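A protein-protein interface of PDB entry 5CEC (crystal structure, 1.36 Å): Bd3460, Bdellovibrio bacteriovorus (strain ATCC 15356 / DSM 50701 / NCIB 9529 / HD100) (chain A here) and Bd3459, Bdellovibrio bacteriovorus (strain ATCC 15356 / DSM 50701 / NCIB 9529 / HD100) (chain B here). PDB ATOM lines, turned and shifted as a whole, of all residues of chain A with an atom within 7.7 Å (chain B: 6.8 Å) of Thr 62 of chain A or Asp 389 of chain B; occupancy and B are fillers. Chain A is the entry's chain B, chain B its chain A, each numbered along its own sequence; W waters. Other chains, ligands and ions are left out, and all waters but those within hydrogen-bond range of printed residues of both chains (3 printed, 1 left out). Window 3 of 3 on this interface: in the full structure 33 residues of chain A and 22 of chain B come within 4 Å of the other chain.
O of Lys 390 of chain B is in hydrogen-bond range of ND2 of Asn 94 of chain A, at 3.0 Å.
The backbone NH of Asp 389 of chain B is in hydrogen-bond range of the side-chain amide oxygen of Asn 362 of chain B (2.8 Å). The guanidinium group (NH1) of Arg 392 of chain B is in hydrogen-bond range of the backbone carbonyl oxygen (O) of Tyr 388 of chain B (3.1 Å). The guanidinium group of Arg 392 of chain B lies within salt-bridge range of the side-chain carboxylate of Asp 389 of chain B (3.98 Å). The side-chain carboxylate (OD1) of Asp 394 of chain B sits at hydrogen-bond distance from the side-chain hydroxyl (OG) of Ser 391 of chain B, 2.7 Å away. N of Met 64 of chain A sits at hydrogen-bond distance from OD1 of Asp 60 of chain A (2.9 Å). N of Asn 94 of chain A sits at hydrogen-bond distance from O of Thr 62 of chain A, at 2.9 Å.
Among the printed residues, pairs that only touch across the chains: Thr 62 of chain A with Lys 390 of chain B (3.6 Å), Thr 62 of chain A with Asp 389 of chain B (3.7 Å), Met 64 of chain A with Arg 392 of chain B (3.8 Å), Phe 102 of chain A with Arg 392 of chain B (3.97 Å) and Asn 94 of chain A with Ser 391 of chain B (3.998 Å).
Of the printed residues of chain A, Asp 389 of chain B touches Thr 62 (3.7 Å). Of the printed residues of chain A, Arg 392 of chain B touches Met 64 and Phe 102. Of the printed residues of chain B, Met 64 of chain A touches Arg 392 (3.8 Å). Printed residues of chain B within 4 Å of Asn 94 of chain A: Lys 390 and Ser 391. Asp 60 of chain A touches none of the printed residues of chain B. Thr 386 of chain B touches none of the printed residues of chain A. The nearest printed residue of chain B that does not touch Thr 62 of chain A is Arg 392 of chain B (4.1 Å). The nearest printed residue of chain A that does not touch Asp 389 of chain B is Glu 61 of chain A (6.0 Å).
Printed residues of chain A that touch a printed residue of chain B: Thr 62, Met 64, Asn 94 and Phe 102. Among the printed residues, no Asp or Glu carboxylate lies within 4 Å of a Lys or Arg side-chain nitrogen of the other chain.
Water W3 lies within hydrogen-bond range of OD2 of Asp 60 of chain A, OG1 of Thr 62 of chain A and NH2 of Arg 392 of chain B. Water W2 lies within hydrogen-bond range of NE of Arg 392 of chain B (2.7 Å), OD1 of Asn 69 of chain A (2.7 Å) and OH of Tyr 388 of chain B (3.2 Å). Water W1 lies within hydrogen-bond range of the side-chain hydroxyl of Thr 62 of chain A (2.8 Å), the side-chain amide oxygen of Asn 94 of chain A (2.8 Å), the backbone NH of Arg 392 of chain B (2.9 Å) and the side-chain amide nitrogen of Asn 93 of chain A (3.0 Å).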
ATOM      1  N   GLN A  59     -13.144 -25.061 -14.410  1.00  0.00           N
ATOM      2  CA  GLN A  59     -12.611 -23.716 -14.474  1.00  0.00           C
ATOM      3  C   GLN A  59     -11.711 -23.430 -13.280  1.00  0.00           C
ATOM      4  O   GLN A  59     -11.966 -23.895 -12.157  1.00  0.00           O
ATOM      5  CB  GLN A  59     -13.762 -22.725 -14.550  1.00  0.00           C
ATOM      6  CG  GLN A  59     -14.465 -22.755 -15.895  1.00  0.00           C
ATOM      7  CD  GLN A  59     -15.799 -22.044 -15.882  1.00  0.00           C
ATOM      8  OE1 GLN A  59     -16.827 -22.604 -15.472  1.00  0.00           O
ATOM      9  NE2 GLN A  59     -15.790 -20.789 -16.301  1.00  0.00           N
ATOM     10  N   ASP A  60     -10.680 -22.623 -13.525  1.00  0.00           N
ATOM     11  CA  ASP A  60      -9.723 -22.284 -12.506  1.00  0.00           C
ATOM     12  C   ASP A  60     -10.192 -21.084 -11.683  1.00  0.00           C
ATOM     13  O   ASP A  60     -11.346 -20.647 -11.807  1.00  0.00           O
ATOM     14  CB  ASP A  60      -8.331 -22.116 -13.121  1.00  0.00           C
ATOM     15  CG  ASP A  60      -8.123 -20.815 -13.856  1.00  0.00           C
ATOM     16  OD1 ASP A  60      -9.020 -19.977 -13.923  1.00  0.00           O
ATOM     17  OD2 ASP A  60      -6.993 -20.644 -14.353  1.00  0.00           O
ATOM     18  N   GLU A  61      -9.301 -20.554 -10.847  1.00  0.00           N
ATOM     19  CA  GLU A  61      -9.669 -19.499  -9.907  1.00  0.00           C
ATOM     20  C   GLU A  61     -10.137 -18.175 -10.533  1.00  0.00           C
ATOM     21  O   GLU A  61     -10.833 -17.415  -9.880  1.00  0.00           O
ATOM     22  CB  GLU A  61      -8.517 -19.235  -8.938  1.00  0.00           C
ATOM     23  CG  GLU A  61      -7.277 -18.624  -9.583  1.00  0.00           C
ATOM     24  CD  GLU A  61      -6.200 -18.259  -8.580  1.00  0.00           C
ATOM     25  OE1 GLU A  61      -6.453 -17.410  -7.692  1.00  0.00           O
ATOM     26  OE2 GLU A  61      -5.096 -18.823  -8.691  1.00  0.00           O
ATOM     27  N   THR A  62      -9.778 -17.914 -11.793  1.00  0.00           N
ATOM     28  CA  THR A  62     -10.283 -16.735 -12.514  1.00  0.00           C
ATOM     29  C   THR A  62     -11.303 -17.096 -13.615  1.00  0.00           C
ATOM     30  O   THR A  62     -11.676 -16.249 -14.410  1.00  0.00           O
ATOM     31  CB  THR A  62      -9.148 -15.872 -13.131  1.00  0.00           C
ATOM     32  OG1 THR A  62      -8.634 -16.471 -14.331  1.00  0.00           O
ATOM     33  CG2 THR A  62      -8.015 -15.636 -12.141  1.00  0.00           C
ATOM     34  N   GLY A  63     -11.759 -18.354 -13.617  1.00  0.00           N
ATOM     35  CA  GLY A  63     -12.796 -18.876 -14.522  1.00  0.00           C
ATOM     36  C   GLY A  63     -12.309 -19.409 -15.840  1.00  0.00           C
ATOM     37  O   GLY A  63     -13.114 -19.647 -16.738  1.00  0.00           O
ATOM     38  N   MET A  64     -10.994 -19.583 -15.986  1.00  0.00           N
ATOM     39  CA  MET A  64     -10.420 -20.045 -17.251  1.00  0.00           C
ATOM     40  C   MET A  64     -10.533 -21.545 -17.418  1.00  0.00           C
ATOM     41  O   MET A  64     -10.368 -22.323 -16.462  1.00  0.00           O
ATOM     42  CB  MET A  64      -8.943 -19.655 -17.349  1.00  0.00           C
ATOM     43  CG  MET A  64      -8.680 -18.159 -17.265  1.00  0.00           C
ATOM     44  SD  MET A  64      -9.272 -17.262 -18.708  1.00  0.00           S
ATOM     45  CE  MET A  64      -8.054 -17.726 -19.937  1.00  0.00           C
ATOM     46  N   THR A  65     -10.731 -21.934 -18.656  1.00  0.00           N
ATOM     47  CA  THR A  65     -10.665 -23.316 -19.116  1.00  0.00           C
ATOM     48  C   THR A  65      -9.461 -23.504 -20.037  1.00  0.00           C
ATOM     49  O   THR A  65      -8.898 -22.533 -20.547  1.00  0.00           O
ATOM     50  CB  THR A  65     -11.885 -23.652 -19.959  1.00  0.00           C
ATOM     51  OG1 THR A  65     -11.928 -22.774 -21.094  1.00  0.00           O
ATOM     52  CG2 THR A  65     -13.170 -23.539 -19.142  1.00  0.00           C
ATOM     53  N   MET A  68     -10.174 -21.675 -23.364  1.00  0.00           N
ATOM     54  CA  MET A  68      -9.922 -20.224 -23.307  1.00  0.00           C
ATOM     55  C   MET A  68      -8.444 -19.917 -23.419  1.00  0.00           C
ATOM     56  O   MET A  68      -8.070 -18.971 -24.112  1.00  0.00           O
ATOM     57  CB  MET A  68     -10.471 -19.611 -22.031  1.00  0.00           C
ATOM     58  CG  MET A  68     -11.981 -19.561 -21.927  1.00  0.00           C
ATOM     59  SD  MET A  68     -12.379 -19.187 -20.208  1.00  0.00           S
ATOM     60  CE  MET A  68     -14.036 -19.828 -20.128  1.00  0.00           C
ATOM     61  N   ASN A  69      -7.624 -20.668 -22.702  1.00  0.00           N
ATOM     62  CA  ASN A  69      -6.192 -20.510 -22.792  1.00  0.00           C
ATOM     63  C   ASN A  69      -5.660 -20.734 -24.199  1.00  0.00           C
ATOM     64  O   ASN A  69      -4.854 -19.941 -24.683  1.00  0.00           O
ATOM     65  CB  ASN A  69      -5.513 -21.463 -21.808  1.00  0.00           C
ATOM     66  CG  ASN A  69      -5.429 -20.907 -20.414  1.00  0.00           C
ATOM     67  OD1 ASN A  69      -4.564 -20.099 -20.131  1.00  0.00           O
ATOM     68  ND2 ASN A  69      -6.317 -21.342 -19.531  1.00  0.00           N
ATOM     69  N   LYS A  92     -17.471 -19.059 -19.393  1.00  0.00           N
ATOM     70  CA  LYS A  92     -16.973 -17.692 -19.325  1.00  0.00           C
ATOM     71  C   LYS A  92     -16.026 -17.510 -18.163  1.00  0.00           C
ATOM     72  O   LYS A  92     -16.234 -18.074 -17.078  1.00  0.00           O
ATOM     73  CB  LYS A  92     -18.128 -16.703 -19.184  1.00  0.00           C
ATOM     74  CG  LYS A  92     -18.980 -16.638 -20.428  1.00  0.00           C
ATOM     75  CD  LYS A  92     -20.225 -15.858 -20.197  1.00  0.00           C
ATOM     76  CE  LYS A  92     -21.081 -15.810 -21.425  1.00  0.00           C
ATOM     77  NZ  LYS A  92     -22.469 -15.458 -21.022  1.00  0.00           N
ATOM     78  N   ASN A  93     -14.976 -16.728 -18.386  1.00  0.00           N
ATOM     79  CA  ASN A  93     -14.078 -16.366 -17.272  1.00  0.00           C
ATOM     80  C   ASN A  93     -14.676 -15.259 -16.421  1.00  0.00           C
ATOM     81  O   ASN A  93     -15.793 -14.821 -16.650  1.00  0.00           O
ATOM     82  CB  ASN A  93     -12.694 -15.993 -17.783  1.00  0.00           C
ATOM     83  CG  ASN A  93     -12.645 -14.595 -18.364  1.00  0.00           C
ATOM     84  OD1 ASN A  93     -13.610 -14.147 -18.965  1.00  0.00           O
ATOM     85  ND2 ASN A  93     -11.555 -13.863 -18.125  1.00  0.00           N
ATOM     86  N   ASN A  94     -13.887 -14.742 -15.485  1.00  0.00           N
ATOM     87  CA  ASN A  94     -14.372 -13.630 -14.640  1.00  0.00           C
ATOM     88  C   ASN A  94     -14.628 -12.319 -15.379  1.00  0.00           C
ATOM     89  O   ASN A  94     -15.427 -11.516 -14.915  1.00  0.00           O
ATOM     90  CB  ASN A  94     -13.485 -13.426 -13.404  1.00  0.00           C
ATOM     91  CG  ASN A  94     -12.061 -12.986 -13.726  1.00  0.00           C
ATOM     92  OD1 ASN A  94     -11.631 -12.973 -14.875  1.00  0.00           O
ATOM     93  ND2 ASN A  94     -11.313 -12.686 -12.698  1.00  0.00           N
ATOM     94  N   GLY A  95     -14.045 -12.169 -16.568  1.00  0.00           N
ATOM     95  CA  GLY A  95     -14.331 -11.052 -17.434  1.00  0.00           C
ATOM     96  C   GLY A  95     -15.536 -11.256 -18.339  1.00  0.00           C
ATOM     97  O   GLY A  95     -15.822 -10.419 -19.183  1.00  0.00           O
ATOM     98  N   GLY A  96     -16.245 -12.363 -18.155  1.00  0.00           N
ATOM     99  CA  GLY A  96     -17.442 -12.647 -18.956  1.00  0.00           C
ATOM    100  C   GLY A  96     -17.204 -13.168 -20.348  1.00  0.00           C
ATOM    101  O   GLY A  96     -18.146 -13.207 -21.145  1.00  0.00           O
ATOM    102  N   PHE A 102     -12.107 -14.520 -26.280  1.00  0.00           N
ATOM    103  CA  PHE A 102     -10.644 -14.511 -26.109  1.00  0.00           C
ATOM    104  C   PHE A 102      -9.918 -14.485 -27.439  1.00  0.00           C
ATOM    105  O   PHE A 102      -8.958 -13.736 -27.605  1.00  0.00           O
ATOM    106  CB  PHE A 102     -10.163 -15.690 -25.275  1.00  0.00           C
ATOM    107  CG  PHE A 102     -10.249 -15.466 -23.808  1.00  0.00           C
ATOM    108  CD1 PHE A 102      -9.271 -14.727 -23.188  1.00  0.00           C
ATOM    109  CD2 PHE A 102     -11.301 -15.966 -23.025  1.00  0.00           C
ATOM    110  CE1 PHE A 102      -9.317 -14.469 -21.837  1.00  0.00           C
ATOM    111  CE2 PHE A 102     -11.314 -15.731 -21.648  1.00  0.00           C
ATOM    112  CZ  PHE A 102     -10.318 -14.986 -21.071  1.00  0.00           C
ATOM    113  N   VAL B 297       6.593 -16.029 -11.006  1.00  0.00           N
ATOM    114  CA  VAL B 297       5.354 -15.336 -10.762  1.00  0.00           C
ATOM    115  C   VAL B 297       5.456 -14.696  -9.358  1.00  0.00           C
ATOM    116  O   VAL B 297       4.979 -13.591  -9.154  1.00  0.00           O
ATOM    117  CB  VAL B 297       4.117 -16.267 -10.883  1.00  0.00           C
ATOM    118  CG1 VAL B 297       2.840 -15.441 -10.870  1.00  0.00           C
ATOM    119  CG2 VAL B 297       4.179 -17.109 -12.159  1.00  0.00           C
ATOM    120  N   TYR B 302      11.356  -8.307 -15.273  1.00  0.00           N
ATOM    121  CA  TYR B 302      11.011  -7.942 -16.658  1.00  0.00           C
ATOM    122  C   TYR B 302      11.965  -6.850 -17.126  1.00  0.00           C
ATOM    123  O   TYR B 302      12.336  -5.955 -16.346  1.00  0.00           O
ATOM    124  CB  TYR B 302       9.575  -7.408 -16.760  1.00  0.00           C
ATOM    125  CG  TYR B 302       8.505  -8.449 -16.511  1.00  0.00           C
ATOM    126  CD1 TYR B 302       8.177  -9.368 -17.472  1.00  0.00           C
ATOM    127  CD2 TYR B 302       7.878  -8.547 -15.268  1.00  0.00           C
ATOM    128  CE1 TYR B 302       7.193 -10.323 -17.267  1.00  0.00           C
ATOM    129  CE2 TYR B 302       6.923  -9.528 -15.023  1.00  0.00           C
ATOM    130  CZ  TYR B 302       6.584 -10.424 -16.030  1.00  0.00           C
ATOM    131  OH  TYR B 302       5.641 -11.405 -15.785  1.00  0.00           O
ATOM    132  N   ASN B 362       2.272 -10.239 -17.851  1.00  0.00           N
ATOM    133  CA  ASN B 362       1.277 -10.138 -16.797  1.00  0.00           C
ATOM    134  C   ASN B 362       0.836  -8.688 -16.545  1.00  0.00           C
ATOM    135  O   ASN B 362      -0.357  -8.371 -16.533  1.00  0.00           O
ATOM    136  CB  ASN B 362       1.843 -10.781 -15.519  1.00  0.00           C
ATOM    137  CG  ASN B 362       0.904 -10.684 -14.339  1.00  0.00           C
ATOM    138  OD1 ASN B 362      -0.300 -10.598 -14.472  1.00  0.00           O
ATOM    139  ND2 ASN B 362       1.478 -10.703 -13.178  1.00  0.00           N
ATOM    140  N   LYS B 363       1.820  -7.818 -16.317  1.00  0.00           N
ATOM    141  CA  LYS B 363       1.539  -6.440 -15.928  1.00  0.00           C
ATOM    142  C   LYS B 363       1.585  -5.413 -17.021  1.00  0.00           C
ATOM    143  O   LYS B 363       1.488  -4.210 -16.731  1.00  0.00           O
ATOM    144  CB  LYS B 363       2.429  -6.010 -14.769  1.00  0.00           C
ATOM    145  CG  LYS B 363       2.310  -6.863 -13.533  1.00  0.00           C
ATOM    146  CD  LYS B 363       0.887  -6.836 -12.981  1.00  0.00           C
ATOM    147  CE  LYS B 363       0.779  -7.389 -11.571  1.00  0.00           C
ATOM    148  NZ  LYS B 363      -0.654  -7.438 -11.122  1.00  0.00           N
ATOM    149  N   THR B 386      -1.646  -3.725 -17.102  1.00  0.00           N
ATOM    150  CA  THR B 386      -2.659  -4.771 -16.982  1.00  0.00           C
ATOM    151  C   THR B 386      -2.445  -5.536 -15.703  1.00  0.00           C
ATOM    152  O   THR B 386      -1.371  -5.440 -15.089  1.00  0.00           O
ATOM    153  CB  THR B 386      -2.611  -5.759 -18.173  1.00  0.00           C
ATOM    154  OG1 THR B 386      -1.309  -6.320 -18.332  1.00  0.00           O
ATOM    155  CG2 THR B 386      -2.934  -5.058 -19.493  1.00  0.00           C
ATOM    156  N   ASP B 387      -3.442  -6.340 -15.323  1.00  0.00           N
ATOM    157  CA  ASP B 387      -3.277  -7.328 -14.229  1.00  0.00           C
ATOM    158  C   ASP B 387      -3.811  -8.671 -14.743  1.00  0.00           C
ATOM    159  O   ASP B 387      -4.856  -9.184 -14.323  1.00  0.00           O
ATOM    160  CB  ASP B 387      -3.978  -6.900 -12.936  1.00  0.00           C
ATOM    161  CG  ASP B 387      -3.492  -5.545 -12.399  1.00  0.00           C
ATOM    162  OD1 ASP B 387      -2.434  -5.485 -11.741  1.00  0.00           O
ATOM    163  OD2 ASP B 387      -4.202  -4.524 -12.611  1.00  0.00           O
ATOM    164  N   TYR B 388      -3.068  -9.221 -15.702  1.00  0.00           N
ATOM    165  CA  TYR B 388      -3.489 -10.425 -16.391  1.00  0.00           C
ATOM    166  C   TYR B 388      -3.663 -11.615 -15.427  1.00  0.00           C
ATOM    167  O   TYR B 388      -4.583 -12.437 -15.625  1.00  0.00           O
ATOM    168  CB  TYR B 388      -2.503 -10.644 -17.533  1.00  0.00           C
ATOM    169  CG  TYR B 388      -2.437 -11.971 -18.173  1.00  0.00           C
ATOM    170  CD1 TYR B 388      -1.683 -13.010 -17.604  1.00  0.00           C
ATOM    171  CD2 TYR B 388      -3.035 -12.185 -19.396  1.00  0.00           C
ATOM    172  CE1 TYR B 388      -1.553 -14.232 -18.247  1.00  0.00           C
ATOM    173  CE2 TYR B 388      -2.897 -13.393 -20.052  1.00  0.00           C
ATOM    174  CZ  TYR B 388      -2.166 -14.416 -19.471  1.00  0.00           C
ATOM    175  OH  TYR B 388      -2.083 -15.628 -20.134  1.00  0.00           O
ATOM    176  N   ASP B 389      -2.862 -11.648 -14.356  1.00  0.00           N
ATOM    177  CA  ASP B 389      -3.034 -12.719 -13.369  1.00  0.00           C
ATOM    178  C   ASP B 389      -4.372 -12.635 -12.589  1.00  0.00           C
ATOM    179  O   ASP B 389      -4.920 -13.691 -12.220  1.00  0.00           O
ATOM    180  CB  ASP B 389      -1.796 -12.873 -12.483  1.00  0.00           C
ATOM    181  CG  ASP B 389      -0.619 -13.501 -13.243  1.00  0.00           C
ATOM    182  OD1 ASP B 389      -0.813 -13.961 -14.393  1.00  0.00           O
ATOM    183  OD2 ASP B 389       0.503 -13.522 -12.705  1.00  0.00           O
ATOM    184  N   LYS B 390      -4.927 -11.441 -12.397  1.00  0.00           N
ATOM    185  CA  LYS B 390      -6.223 -11.270 -11.737  1.00  0.00           C
ATOM    186  C   LYS B 390      -7.340 -11.485 -12.767  1.00  0.00           C
ATOM    187  O   LYS B 390      -8.394 -12.024 -12.456  1.00  0.00           O
ATOM    188  CB  LYS B 390      -6.358  -9.864 -11.115  1.00  0.00           C
ATOM    189  CG  LYS B 390      -5.468  -9.557  -9.905  1.00  0.00           C
ATOM    190  CD  LYS B 390      -5.950 -10.281  -8.654  1.00  0.00           C
ATOM    191  CE  LYS B 390      -5.159  -9.904  -7.404  1.00  0.00           C
ATOM    192  NZ  LYS B 390      -3.701 -10.184  -7.542  1.00  0.00           N
ATOM    193  N   SER B 391      -7.097 -11.030 -13.991  1.00  0.00           N
ATOM    194  CA  SER B 391      -8.113 -11.079 -15.010  1.00  0.00           C
ATOM    195  C   SER B 391      -7.496 -11.204 -16.377  1.00  0.00           C
ATOM    196  O   SER B 391      -6.945 -10.255 -16.940  1.00  0.00           O
ATOM    197  CB  SER B 391      -9.026  -9.868 -14.922  1.00  0.00           C
ATOM    198  OG  SER B 391      -8.338  -8.725 -15.246  1.00  0.00           O
ATOM    199  N   ARG B 392      -7.615 -12.396 -16.929  1.00  0.00           N
ATOM    200  CA  ARG B 392      -6.959 -12.702 -18.210  1.00  0.00           C
ATOM    201  C   ARG B 392      -7.541 -11.870 -19.332  1.00  0.00           C
ATOM    202  O   ARG B 392      -6.877 -11.721 -20.340  1.00  0.00           O
ATOM    203  CB  ARG B 392      -7.086 -14.197 -18.508  1.00  0.00           C
ATOM    204  CG  ARG B 392      -6.427 -15.079 -17.460  1.00  0.00           C
ATOM    205  CD  ARG B 392      -4.936 -15.150 -17.580  1.00  0.00           C
ATOM    206  NE  ARG B 392      -4.402 -16.308 -16.837  1.00  0.00           N
ATOM    207  CZ  ARG B 392      -4.212 -16.394 -15.513  1.00  0.00           C
ATOM    208  NH1 ARG B 392      -4.507 -15.405 -14.678  1.00  0.00           N
ATOM    209  NH2 ARG B 392      -3.697 -17.492 -15.014  1.00  0.00           N
ATOM    210  N   ASP B 394      -7.780  -8.772 -19.455  1.00  0.00           N
ATOM    211  CA  ASP B 394      -7.104  -7.461 -19.531  1.00  0.00           C
ATOM    212  C   ASP B 394      -6.295  -7.282 -20.803  1.00  0.00           C
ATOM    213  O   ASP B 394      -6.238  -6.162 -21.278  1.00  0.00           O
ATOM    214  CB  ASP B 394      -6.181  -7.230 -18.328  1.00  0.00           C
ATOM    215  CG  ASP B 394      -6.882  -6.790 -17.073  1.00  0.00           C
ATOM    216  OD1 ASP B 394      -8.135  -6.757 -17.023  1.00  0.00           O
ATOM    217  OD2 ASP B 394      -6.131  -6.431 -16.118  1.00  0.00           O
HETATM  218  O   HOH W   1      -9.522 -14.425 -16.013  1.00  0.00           O
HETATM  219  O   HOH W   2      -4.296 -17.640 -19.142  1.00  0.00           O
HETATM  220  O   HOH W   3      -6.560 -18.082 -13.860  1.00  0.00           O
